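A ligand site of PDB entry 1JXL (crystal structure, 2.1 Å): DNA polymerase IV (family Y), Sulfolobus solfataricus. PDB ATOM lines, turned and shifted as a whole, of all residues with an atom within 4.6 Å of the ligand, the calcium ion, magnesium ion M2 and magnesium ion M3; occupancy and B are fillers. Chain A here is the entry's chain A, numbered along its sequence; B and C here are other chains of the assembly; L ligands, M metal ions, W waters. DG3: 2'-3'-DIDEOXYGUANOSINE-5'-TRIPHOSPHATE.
The side-chain amino group of Lys 152 is in salt-bridge range of the side-chain carboxylate of Glu 106, at 3.1 Å. The side-chain carboxylate (OD2) of Asp 7 lies within salt-bridge range of the side-chain amino group (NZ) of Lys 159, 3.2 Å away. NH2 of Arg 51 sits at hydrogen-bond distance from OG1 of Thr 45 (3.2 Å). The backbone NH (N) of Gly 58 lies within hydrogen-bond range of the backbone carbonyl oxygen (O) of Val 43, 2.8 Å away.
An oxygen (O3G) of the ligand is in hydrogen-bond range of the side-chain hydroxyl (OG1) of Thr 45 (2.6 Å). NH2 of Arg 51 lies within salt-bridge range of O3G of the ligand (3.4 Å). N2 of the ligand lies within hydrogen-bond range of O2 of DC 3 of chain B, at 2.7 Å. The backbone NH (N) of Phe 11 lies close to an oxygen (O2G) of the ligand (3.2 Å). The backbone NH (N) of Tyr 10 lies close to an oxygen (O2G) of the ligand. The side-chain amino group (NZ) of Lys 159 sits close to an oxygen (O2B) of the ligand.
An oxygen (O1G) of the ligand is bound to magnesium ion M3, at 1.9 Å. Magnesium ion M3 is bound by water W4 (2.0 Å). O1B of the ligand binds magnesium ion M3, 2.4 Å away. Magnesium ion M3 has three donor atoms within binding distance. Slightly farther from magnesium ion M3 lies water W7 (2.7 Å).
Water W8 lies within hydrogen-bond range of O3G of the ligand (2.8 Å) and N of Tyr 12 of chain A (3.0 Å). Water W2 lies within hydrogen-bond range of O3G of the ligand (2.8 Å), OG1 of Thr 45 (3.0 Å) and NH2 of Arg 51 (3.4 Å). Water W3 lies within hydrogen-bond range of the side-chain hydroxyl of Tyr 12 of chain A (2.8 Å) and a nitrogen (N3) of the ligand (2.9 Å).
Tyr 10 touches magnesium ion M3 (N to MG, 3.8 Å). Arg 51 touches magnesium ion M3. Lys 159 touches magnesium ion M3 (NZ to MG, 3.8 Å). Of the 21 residues printed, 3 come within 4 Å of magnesium ion M3. The nearest printed residue that does not touch magnesium ion M3 is Tyr 48 (4.04 Å).
Three residues have an atom within 4 Å of the calcium ion: Asp 7, Phe 8 and Asp 105.
O2A of the ligand sits close to O3' of DT 12 of chain C. Merely in contact with the ligand: Ala 57, Ala 44, DG 4 of chain B and Gly 58. Hydrophobic or aromatic side chains within 4 Å of the ligand: Ala 44 and Ala 57. 15 residues have an atom within 4 Å of the ligand: Asp 7, Phe 8, Tyr 10, Phe 11, Ala 44, Thr 45, Arg 51, Ala 57, Gly 58, Asp 105, Glu 106, Lys 159, DC 3 of chain B, DG 4 of chain B and DT 12 of chain C.
Magnesium ion M2 is bound by OE2 of Glu 106 (1.9 Å). O2B of the ligand is bound to magnesium ion M2, 2.2 Å away. Magnesium ion M2 has two donor atoms within binding distance. Slightly farther from magnesium ion M2 lies the side-chain carboxylate (OD2) of Asp 7 (2.6 Å).
Within 4 Å of magnesium ion M2: Asp 7, Asp 105 and Glu 106. The nearest printed residue that does not touch magnesium ion M2 is Lys 159 (4.3 Å).
The calcium ion is bound by the side-chain carboxylate of Asp 105 (2.3 Å), the side-chain carboxylate of Asp 7 (2.3 Å), an oxygen (O2G) of the ligand (2.3 Å), water W4 (2.4 Å), the backbone carbonyl oxygen of Phe 8 (2.4 Å) and an oxygen (O2B) of the ligand (2.5 Å).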
ATOM      1  N   ASP A   7      10.811 -10.287  -2.410  1.00  0.00           N
ATOM      2  CA  ASP A   7       9.650  -9.779  -1.708  1.00  0.00           C
ATOM      3  C   ASP A   7       8.419 -10.538  -2.217  1.00  0.00           C
ATOM      4  O   ASP A   7       8.009 -10.381  -3.379  1.00  0.00           O
ATOM      5  CB  ASP A   7       9.490  -8.298  -2.023  1.00  0.00           C
ATOM      6  CG  ASP A   7       8.389  -7.641  -1.223  1.00  0.00           C
ATOM      7  OD1 ASP A   7       7.237  -8.158  -1.163  1.00  0.00           O
ATOM      8  OD2 ASP A   7       8.675  -6.550  -0.671  1.00  0.00           O
ATOM      9  N   PHE A   8       7.789 -11.349  -1.350  1.00  0.00           N
ATOM     10  CA  PHE A   8       6.646 -12.120  -1.854  1.00  0.00           C
ATOM     11  C   PHE A   8       5.425 -11.235  -2.187  1.00  0.00           C
ATOM     12  O   PHE A   8       5.029 -10.438  -1.380  1.00  0.00           O
ATOM     13  CB  PHE A   8       6.238 -13.178  -0.820  1.00  0.00           C
ATOM     14  CG  PHE A   8       7.395 -13.903  -0.160  1.00  0.00           C
ATOM     15  CD1 PHE A   8       8.608 -14.081  -0.811  1.00  0.00           C
ATOM     16  CD2 PHE A   8       7.217 -14.508   1.080  1.00  0.00           C
ATOM     17  CE1 PHE A   8       9.608 -14.838  -0.263  1.00  0.00           C
ATOM     18  CE2 PHE A   8       8.236 -15.295   1.627  1.00  0.00           C
ATOM     19  CZ  PHE A   8       9.430 -15.444   0.940  1.00  0.00           C
ATOM     20  N   ASP A   9       4.807 -11.398  -3.344  1.00  0.00           N
ATOM     21  CA  ASP A   9       3.654 -10.558  -3.688  1.00  0.00           C
ATOM     22  C   ASP A   9       2.379 -10.707  -2.833  1.00  0.00           C
ATOM     23  O   ASP A   9       1.929 -11.820  -2.588  1.00  0.00           O
ATOM     24  CB  ASP A   9       3.265 -10.768  -5.162  1.00  0.00           C
ATOM     25  CG  ASP A   9       4.467 -10.571  -6.141  1.00  0.00           C
ATOM     26  OD1 ASP A   9       5.241  -9.609  -5.969  1.00  0.00           O
ATOM     27  OD2 ASP A   9       4.615 -11.358  -7.100  1.00  0.00           O
ATOM     28  N   TYR A  10       1.791  -9.585  -2.408  1.00  0.00           N
ATOM     29  CA  TYR A  10       0.563  -9.573  -1.603  1.00  0.00           C
ATOM     30  C   TYR A  10       0.474 -10.888  -0.764  1.00  0.00           C
ATOM     31  O   TYR A  10      -0.576 -11.566  -0.740  1.00  0.00           O
ATOM     32  CB  TYR A  10      -0.669  -9.326  -2.559  1.00  0.00           C
ATOM     33  CG  TYR A  10      -0.985 -10.352  -3.663  1.00  0.00           C
ATOM     34  CD1 TYR A  10      -2.016 -11.305  -3.493  1.00  0.00           C
ATOM     35  CD2 TYR A  10      -0.258 -10.388  -4.877  1.00  0.00           C
ATOM     36  CE1 TYR A  10      -2.321 -12.281  -4.506  1.00  0.00           C
ATOM     37  CE2 TYR A  10      -0.559 -11.362  -5.902  1.00  0.00           C
ATOM     38  CZ  TYR A  10      -1.587 -12.293  -5.699  1.00  0.00           C
ATOM     39  OH  TYR A  10      -1.912 -13.220  -6.701  1.00  0.00           O
ATOM     40  N   PHE A  11       1.608 -11.249  -0.118  1.00  0.00           N
ATOM     41  CA  PHE A  11       1.702 -12.487   0.626  1.00  0.00           C
ATOM     42  C   PHE A  11       0.529 -13.142   1.294  1.00  0.00           C
ATOM     43  O   PHE A  11       0.180 -14.258   0.891  1.00  0.00           O
ATOM     44  CB  PHE A  11       2.895 -12.442   1.618  1.00  0.00           C
ATOM     45  CG  PHE A  11       3.400 -13.824   1.980  1.00  0.00           C
ATOM     46  CD1 PHE A  11       3.545 -14.778   0.993  1.00  0.00           C
ATOM     47  CD2 PHE A  11       3.604 -14.202   3.319  1.00  0.00           C
ATOM     48  CE1 PHE A  11       3.905 -16.096   1.321  1.00  0.00           C
ATOM     49  CE2 PHE A  11       3.973 -15.528   3.663  1.00  0.00           C
ATOM     50  CZ  PHE A  11       4.109 -16.474   2.660  1.00  0.00           C
ATOM     51  N   TYR A  12      -0.100 -12.474   2.264  1.00  0.00           N
ATOM     52  CA  TYR A  12      -1.237 -13.057   2.983  1.00  0.00           C
ATOM     53  C   TYR A  12      -2.428 -13.395   2.063  1.00  0.00           C
ATOM     54  O   TYR A  12      -2.915 -14.514   2.127  1.00  0.00           O
ATOM     55  CB  TYR A  12      -1.726 -12.187   4.155  1.00  0.00           C
ATOM     56  CG  TYR A  12      -0.690 -11.817   5.217  1.00  0.00           C
ATOM     57  CD1 TYR A  12       0.581 -12.377   5.201  1.00  0.00           C
ATOM     58  CD2 TYR A  12      -0.988 -10.880   6.236  1.00  0.00           C
ATOM     59  CE1 TYR A  12       1.548 -12.040   6.151  1.00  0.00           C
ATOM     60  CE2 TYR A  12      -0.020 -10.513   7.198  1.00  0.00           C
ATOM     61  CZ  TYR A  12       1.261 -11.109   7.135  1.00  0.00           C
ATOM     62  OH  TYR A  12       2.265 -10.748   8.024  1.00  0.00           O
ATOM     63  N   VAL A  32      -7.822  -7.919   9.979  1.00  0.00           N
ATOM     64  CA  VAL A  32      -7.533  -8.104  11.386  1.00  0.00           C
ATOM     65  C   VAL A  32      -8.760  -7.549  12.086  1.00  0.00           C
ATOM     66  O   VAL A  32      -8.891  -6.306  12.228  1.00  0.00           O
ATOM     67  CB  VAL A  32      -6.331  -7.275  11.833  1.00  0.00           C
ATOM     68  CG1 VAL A  32      -6.095  -7.479  13.348  1.00  0.00           C
ATOM     69  CG2 VAL A  32      -5.108  -7.668  11.025  1.00  0.00           C
ATOM     70  N   VAL A  43      -7.583  -3.587   7.575  1.00  0.00           N
ATOM     71  CA  VAL A  43      -7.197  -4.434   6.461  1.00  0.00           C
ATOM     72  C   VAL A  43      -5.698  -4.666   6.631  1.00  0.00           C
ATOM     73  O   VAL A  43      -4.937  -3.687   6.669  1.00  0.00           O
ATOM     74  CB  VAL A  43      -7.383  -3.735   5.127  1.00  0.00           C
ATOM     75  CG1 VAL A  43      -6.575  -4.501   4.069  1.00  0.00           C
ATOM     76  CG2 VAL A  43      -8.919  -3.617   4.773  1.00  0.00           C
ATOM     77  N   ALA A  44      -5.294  -5.938   6.756  1.00  0.00           N
ATOM     78  CA  ALA A  44      -3.865  -6.325   6.905  1.00  0.00           C
ATOM     79  C   ALA A  44      -3.230  -6.258   5.507  1.00  0.00           C
ATOM     80  O   ALA A  44      -2.118  -5.686   5.334  1.00  0.00           O
ATOM     81  CB  ALA A  44      -3.739  -7.799   7.494  1.00  0.00           C
ATOM     82  N   THR A  45      -3.886  -6.891   4.524  1.00  0.00           N
ATOM     83  CA  THR A  45      -3.430  -6.774   3.153  1.00  0.00           C
ATOM     84  C   THR A  45      -4.498  -7.158   2.103  1.00  0.00           C
ATOM     85  O   THR A  45      -5.466  -7.787   2.415  1.00  0.00           O
ATOM     86  CB  THR A  45      -2.184  -7.614   2.894  1.00  0.00           C
ATOM     87  OG1 THR A  45      -1.740  -7.347   1.552  1.00  0.00           O
ATOM     88  CG2 THR A  45      -2.496  -9.066   2.973  1.00  0.00           C
ATOM     89  N   TYR A  48      -4.104  -7.506  -5.689  1.00  0.00           N
ATOM     90  CA  TYR A  48      -4.184  -6.446  -6.702  1.00  0.00           C
ATOM     91  C   TYR A  48      -5.580  -6.060  -7.146  1.00  0.00           C
ATOM     92  O   TYR A  48      -5.850  -4.882  -7.317  1.00  0.00           O
ATOM     93  CB  TYR A  48      -3.308  -6.785  -7.895  1.00  0.00           C
ATOM     94  CG  TYR A  48      -1.870  -6.595  -7.488  1.00  0.00           C
ATOM     95  CD1 TYR A  48      -1.144  -7.653  -6.913  1.00  0.00           C
ATOM     96  CD2 TYR A  48      -1.299  -5.325  -7.491  1.00  0.00           C
ATOM     97  CE1 TYR A  48       0.091  -7.427  -6.347  1.00  0.00           C
ATOM     98  CE2 TYR A  48      -0.065  -5.093  -6.947  1.00  0.00           C
ATOM     99  CZ  TYR A  48       0.612  -6.142  -6.375  1.00  0.00           C
ATOM    100  OH  TYR A  48       1.848  -5.840  -5.811  1.00  0.00           O
ATOM    101  N   ARG A  51      -6.660  -3.852  -4.421  1.00  0.00           N
ATOM    102  CA  ARG A  51      -5.878  -2.597  -4.378  1.00  0.00           C
ATOM    103  C   ARG A  51      -6.186  -1.687  -5.541  1.00  0.00           C
ATOM    104  O   ARG A  51      -6.186  -0.496  -5.388  1.00  0.00           O
ATOM    105  CB  ARG A  51      -4.353  -2.876  -4.320  1.00  0.00           C
ATOM    106  CG  ARG A  51      -3.932  -3.513  -3.017  1.00  0.00           C
ATOM    107  CD  ARG A  51      -2.635  -3.033  -2.416  1.00  0.00           C
ATOM    108  NE  ARG A  51      -2.101  -4.180  -1.684  1.00  0.00           N
ATOM    109  CZ  ARG A  51      -0.816  -4.490  -1.500  1.00  0.00           C
ATOM    110  NH1 ARG A  51       0.135  -3.728  -2.003  1.00  0.00           N
ATOM    111  NH2 ARG A  51      -0.486  -5.562  -0.764  1.00  0.00           N
ATOM    112  N   ALA A  57      -3.787  -2.175   2.796  1.00  0.00           N
ATOM    113  CA  ALA A  57      -3.358  -2.325   4.200  1.00  0.00           C
ATOM    114  C   ALA A  57      -3.549  -0.991   4.933  1.00  0.00           C
ATOM    115  O   ALA A  57      -3.243   0.081   4.378  1.00  0.00           O
ATOM    116  CB  ALA A  57      -1.852  -2.719   4.265  1.00  0.00           C
ATOM    117  N   GLY A  58      -4.095  -1.065   6.139  1.00  0.00           N
ATOM    118  CA  GLY A  58      -4.253   0.140   6.941  1.00  0.00           C
ATOM    119  C   GLY A  58      -5.633   0.761   7.049  1.00  0.00           C
ATOM    120  O   GLY A  58      -5.933   1.368   8.073  1.00  0.00           O
ATOM    121  N   ASP A 105       7.840 -11.769   4.682  1.00  0.00           N
ATOM    122  CA  ASP A 105       7.830 -11.906   3.223  1.00  0.00           C
ATOM    123  C   ASP A 105       8.975 -11.242   2.475  1.00  0.00           C
ATOM    124  O   ASP A 105       8.800 -10.912   1.321  1.00  0.00           O
ATOM    125  CB  ASP A 105       6.508 -11.376   2.666  1.00  0.00           C
ATOM    126  CG  ASP A 105       6.485  -9.906   2.666  1.00  0.00           C
ATOM    127  OD1 ASP A 105       7.041  -9.408   3.630  1.00  0.00           O
ATOM    128  OD2 ASP A 105       5.977  -9.281   1.745  1.00  0.00           O
ATOM    129  N   GLU A 106      10.124 -11.029   3.135  1.00  0.00           N
ATOM    130  CA  GLU A 106      11.264 -10.361   2.504  1.00  0.00           C
ATOM    131  C   GLU A 106      12.607 -10.953   2.931  1.00  0.00           C
ATOM    132  O   GLU A 106      12.828 -11.225   4.136  1.00  0.00           O
ATOM    133  CB  GLU A 106      11.268  -8.883   2.904  1.00  0.00           C
ATOM    134  CG  GLU A 106      10.081  -8.129   2.388  1.00  0.00           C
ATOM    135  CD  GLU A 106      10.161  -6.651   2.719  1.00  0.00           C
ATOM    136  OE1 GLU A 106      11.240  -6.170   3.159  1.00  0.00           O
ATOM    137  OE2 GLU A 106       9.155  -5.956   2.508  1.00  0.00           O
ATOM    138  N   LYS A 152      16.032  -3.157  -2.761  1.00  0.00           N
ATOM    139  CA  LYS A 152      14.641  -3.082  -2.306  1.00  0.00           C
ATOM    140  C   LYS A 152      13.896  -2.087  -3.164  1.00  0.00           C
ATOM    141  O   LYS A 152      12.753  -2.327  -3.552  1.00  0.00           O
ATOM    142  CB  LYS A 152      14.577  -2.635  -0.832  1.00  0.00           C
ATOM    143  CG  LYS A 152      13.148  -2.364  -0.275  1.00  0.00           C
ATOM    144  CD  LYS A 152      13.150  -2.493   1.288  1.00  0.00           C
ATOM    145  CE  LYS A 152      11.753  -2.468   1.947  1.00  0.00           C
ATOM    146  NZ  LYS A 152      10.872  -3.611   1.526  1.00  0.00           N
ATOM    147  N   LYS A 159       7.325  -4.424  -8.576  1.00  0.00           N
ATOM    148  CA  LYS A 159       6.228  -5.280  -8.134  1.00  0.00           C
ATOM    149  C   LYS A 159       4.950  -4.937  -8.842  1.00  0.00           C
ATOM    150  O   LYS A 159       4.704  -3.799  -9.146  1.00  0.00           O
ATOM    151  CB  LYS A 159       6.077  -5.259  -6.587  1.00  0.00           C
ATOM    152  CG  LYS A 159       5.705  -3.940  -5.920  1.00  0.00           C
ATOM    153  CD  LYS A 159       5.478  -4.141  -4.384  1.00  0.00           C
ATOM    154  CE  LYS A 159       6.740  -4.625  -3.621  1.00  0.00           C
ATOM    155  NZ  LYS A 159       6.556  -4.654  -2.128  1.00  0.00           N
ATOM    156  P    DC B   3      -9.550  -1.341  16.006  1.00  0.00           P
ATOM    157  OP1  DC B   3     -10.787  -1.867  16.648  1.00  0.00           O
ATOM    158  OP2  DC B   3      -8.646  -0.420  16.744  1.00  0.00           O
ATOM    159  O5'  DC B   3      -8.719  -2.617  15.568  1.00  0.00           O
ATOM    160  C5'  DC B   3      -7.714  -2.520  14.582  1.00  0.00           C
ATOM    161  C4'  DC B   3      -6.973  -3.828  14.530  1.00  0.00           C
ATOM    162  O4'  DC B   3      -6.194  -3.942  13.325  1.00  0.00           O
ATOM    163  C3'  DC B   3      -6.008  -4.047  15.679  1.00  0.00           C
ATOM    164  O3'  DC B   3      -6.044  -5.449  15.971  1.00  0.00           O
ATOM    165  C2'  DC B   3      -4.670  -3.586  15.097  1.00  0.00           C
ATOM    166  C1'  DC B   3      -4.815  -3.928  13.607  1.00  0.00           C
ATOM    167  N1   DC B   3      -4.213  -2.949  12.685  1.00  0.00           N
ATOM    168  C2   DC B   3      -3.274  -3.376  11.738  1.00  0.00           C
ATOM    169  O2   DC B   3      -2.991  -4.596  11.670  1.00  0.00           O
ATOM    170  N3   DC B   3      -2.715  -2.438  10.910  1.00  0.00           N
ATOM    171  C4   DC B   3      -3.077  -1.152  11.006  1.00  0.00           C
ATOM    172  N4   DC B   3      -2.503  -0.280  10.201  1.00  0.00           N
ATOM    173  C5   DC B   3      -4.041  -0.714  11.948  1.00  0.00           C
ATOM    174  C6   DC B   3      -4.586  -1.629  12.754  1.00  0.00           C
ATOM    175  P    DG B   4      -5.337  -6.011  17.294  1.00  0.00           P
ATOM    176  OP1  DG B   4      -5.927  -7.345  17.614  1.00  0.00           O
ATOM    177  OP2  DG B   4      -5.352  -4.932  18.327  1.00  0.00           O
ATOM    178  O5'  DG B   4      -3.857  -6.242  16.801  1.00  0.00           O
ATOM    179  C5'  DG B   4      -3.594  -7.201  15.792  1.00  0.00           C
ATOM    180  C4'  DG B   4      -2.136  -7.163  15.440  1.00  0.00           C
ATOM    181  O4'  DG B   4      -1.815  -6.036  14.565  1.00  0.00           O
ATOM    182  C3'  DG B   4      -1.261  -6.999  16.686  1.00  0.00           C
ATOM    183  O3'  DG B   4      -0.156  -7.833  16.524  1.00  0.00           O
ATOM    184  C2'  DG B   4      -0.795  -5.564  16.623  1.00  0.00           C
ATOM    185  C1'  DG B   4      -0.724  -5.312  15.114  1.00  0.00           C
ATOM    186  N9   DG B   4      -0.858  -3.911  14.733  1.00  0.00           N
ATOM    187  C8   DG B   4      -1.546  -2.940  15.418  1.00  0.00           C
ATOM    188  N7   DG B   4      -1.438  -1.754  14.881  1.00  0.00           N
ATOM    189  C5   DG B   4      -0.650  -1.950  13.769  1.00  0.00           C
ATOM    190  C6   DG B   4      -0.202  -1.017  12.778  1.00  0.00           C
ATOM    191  O6   DG B   4      -0.440   0.203  12.696  1.00  0.00           O
ATOM    192  N1   DG B   4       0.588  -1.629  11.829  1.00  0.00           N
ATOM    193  C2   DG B   4       0.898  -2.961  11.816  1.00  0.00           C
ATOM    194  N2   DG B   4       1.664  -3.342  10.816  1.00  0.00           N
ATOM    195  N3   DG B   4       0.481  -3.848  12.712  1.00  0.00           N
ATOM    196  C4   DG B   4      -0.286  -3.276  13.653  1.00  0.00           C
ATOM    197  P    DT C  12       9.235   2.995   5.902  1.00  0.00           P
ATOM    198  OP1  DT C  12      10.225   3.136   4.808  1.00  0.00           O
ATOM    199  OP2  DT C  12       7.939   3.710   5.781  1.00  0.00           O
ATOM    200  O5'  DT C  12       8.941   1.453   6.089  1.00  0.00           O
ATOM    201  C5'  DT C  12       9.979   0.525   6.472  1.00  0.00           C
ATOM    202  C4'  DT C  12       9.381  -0.856   6.649  1.00  0.00           C
ATOM    203  O4'  DT C  12       8.717  -0.963   7.945  1.00  0.00           O
ATOM    204  C3'  DT C  12       8.329  -1.236   5.604  1.00  0.00           C
ATOM    205  O3'  DT C  12       8.534  -2.580   5.147  1.00  0.00           O
ATOM    206  C2'  DT C  12       7.020  -1.147   6.355  1.00  0.00           C
ATOM    207  C1'  DT C  12       7.432  -1.535   7.769  1.00  0.00           C
ATOM    208  N1   DT C  12       6.579  -1.044   8.897  1.00  0.00           N
ATOM    209  C2   DT C  12       6.521  -1.820  10.074  1.00  0.00           C
ATOM    210  O2   DT C  12       7.148  -2.850  10.259  1.00  0.00           O
ATOM    211  N3   DT C  12       5.696  -1.320  11.040  1.00  0.00           N
ATOM    212  C4   DT C  12       4.980  -0.153  11.009  1.00  0.00           C
ATOM    213  O4   DT C  12       4.298   0.151  11.974  1.00  0.00           O
ATOM    214  C5   DT C  12       5.109   0.634   9.771  1.00  0.00           C
ATOM    215  C7   DT C  12       4.387   1.946   9.651  1.00  0.00           C
ATOM    216  C6   DT C  12       5.873   0.128   8.788  1.00  0.00           C
HETATM  217  PG  DG3 L   1       2.210  -7.222   0.733  1.00  0.00           P
HETATM  218  O1G DG3 L   1       2.005  -6.196  -0.310  1.00  0.00           O
HETATM  219  O2G DG3 L   1       3.006  -8.477   0.438  1.00  0.00           O
HETATM  220  O3G DG3 L   1       0.858  -7.593   1.541  1.00  0.00           O
HETATM  221  O3B DG3 L   1       3.056  -6.199   1.628  1.00  0.00           O
HETATM  222  PB  DG3 L   1       4.258  -5.319   1.025  1.00  0.00           P
HETATM  223  O1B DG3 L   1       3.573  -4.582  -0.027  1.00  0.00           O
HETATM  224  O2B DG3 L   1       5.465  -6.135   0.900  1.00  0.00           O
HETATM  225  O3A DG3 L   1       4.355  -4.289   2.258  1.00  0.00           O
HETATM  226  PA  DG3 L   1       5.213  -4.169   3.655  1.00  0.00           P
HETATM  227  O1A DG3 L   1       4.703  -2.810   4.071  1.00  0.00           O
HETATM  228  O2A DG3 L   1       6.679  -4.406   3.380  1.00  0.00           O
HETATM  229  O5' DG3 L   1       4.704  -5.299   4.688  1.00  0.00           O
HETATM  230  C5' DG3 L   1       5.147  -6.674   4.902  1.00  0.00           C
HETATM  231  C4' DG3 L   1       4.045  -7.482   5.594  1.00  0.00           C
HETATM  232  O4' DG3 L   1       3.232  -6.686   6.544  1.00  0.00           O
HETATM  233  C3' DG3 L   1       3.018  -8.127   4.646  1.00  0.00           C
HETATM  234  C2' DG3 L   1       1.826  -7.165   4.695  1.00  0.00           C
HETATM  235  C1' DG3 L   1       1.858  -6.663   6.152  1.00  0.00           C
HETATM  236  N9  DG3 L   1       1.384  -5.297   6.401  1.00  0.00           N
HETATM  237  C8  DG3 L   1       1.619  -4.107   5.706  1.00  0.00           C
HETATM  238  N7  DG3 L   1       0.993  -3.056   6.205  1.00  0.00           N
HETATM  239  C5  DG3 L   1       0.233  -3.620   7.240  1.00  0.00           C
HETATM  240  C6  DG3 L   1      -0.792  -3.064   8.111  1.00  0.00           C
HETATM  241  O6  DG3 L   1      -1.165  -1.883   8.076  1.00  0.00           O
HETATM  242  N1  DG3 L   1      -1.348  -3.999   9.051  1.00  0.00           N
HETATM  243  C2  DG3 L   1      -0.932  -5.337   9.161  1.00  0.00           C
HETATM  244  N2  DG3 L   1      -1.486  -6.147  10.085  1.00  0.00           N
HETATM  245  N3  DG3 L   1       0.018  -5.851   8.366  1.00  0.00           N
HETATM  246  C4  DG3 L   1       0.539  -4.974   7.444  1.00  0.00           C
HETATM  247 CA    CA M   1       5.213  -8.370  -0.166  1.00  0.00          CA
HETATM  248 MG    MG M   2       7.503  -6.536   1.665  1.00  0.00          MG
HETATM  249 MG    MG M   3       2.971  -5.986  -1.932  1.00  0.00          MG
HETATM  250  O   HOH W   1       1.854  -3.098   1.787  1.00  0.00           O
HETATM  251  O   HOH W   2       0.009  -5.107   2.551  1.00  0.00           O
HETATM  252  O   HOH W   3       1.295  -8.305   9.122  1.00  0.00           O
HETATM  253  O   HOH W   4       4.796  -6.855  -1.941  1.00  0.00           O
HETATM  254  O   HOH W   5       2.862  -2.069  -0.433  1.00  0.00           O
HETATM  255  O   HOH W   6       7.977  -6.129   5.108  1.00  0.00           O
HETATM  256  O   HOH W   7       3.212  -3.333  -2.474  1.00  0.00           O
HETATM  257  O   HOH W   8       0.871  -9.831   3.169  1.00  0.00           O
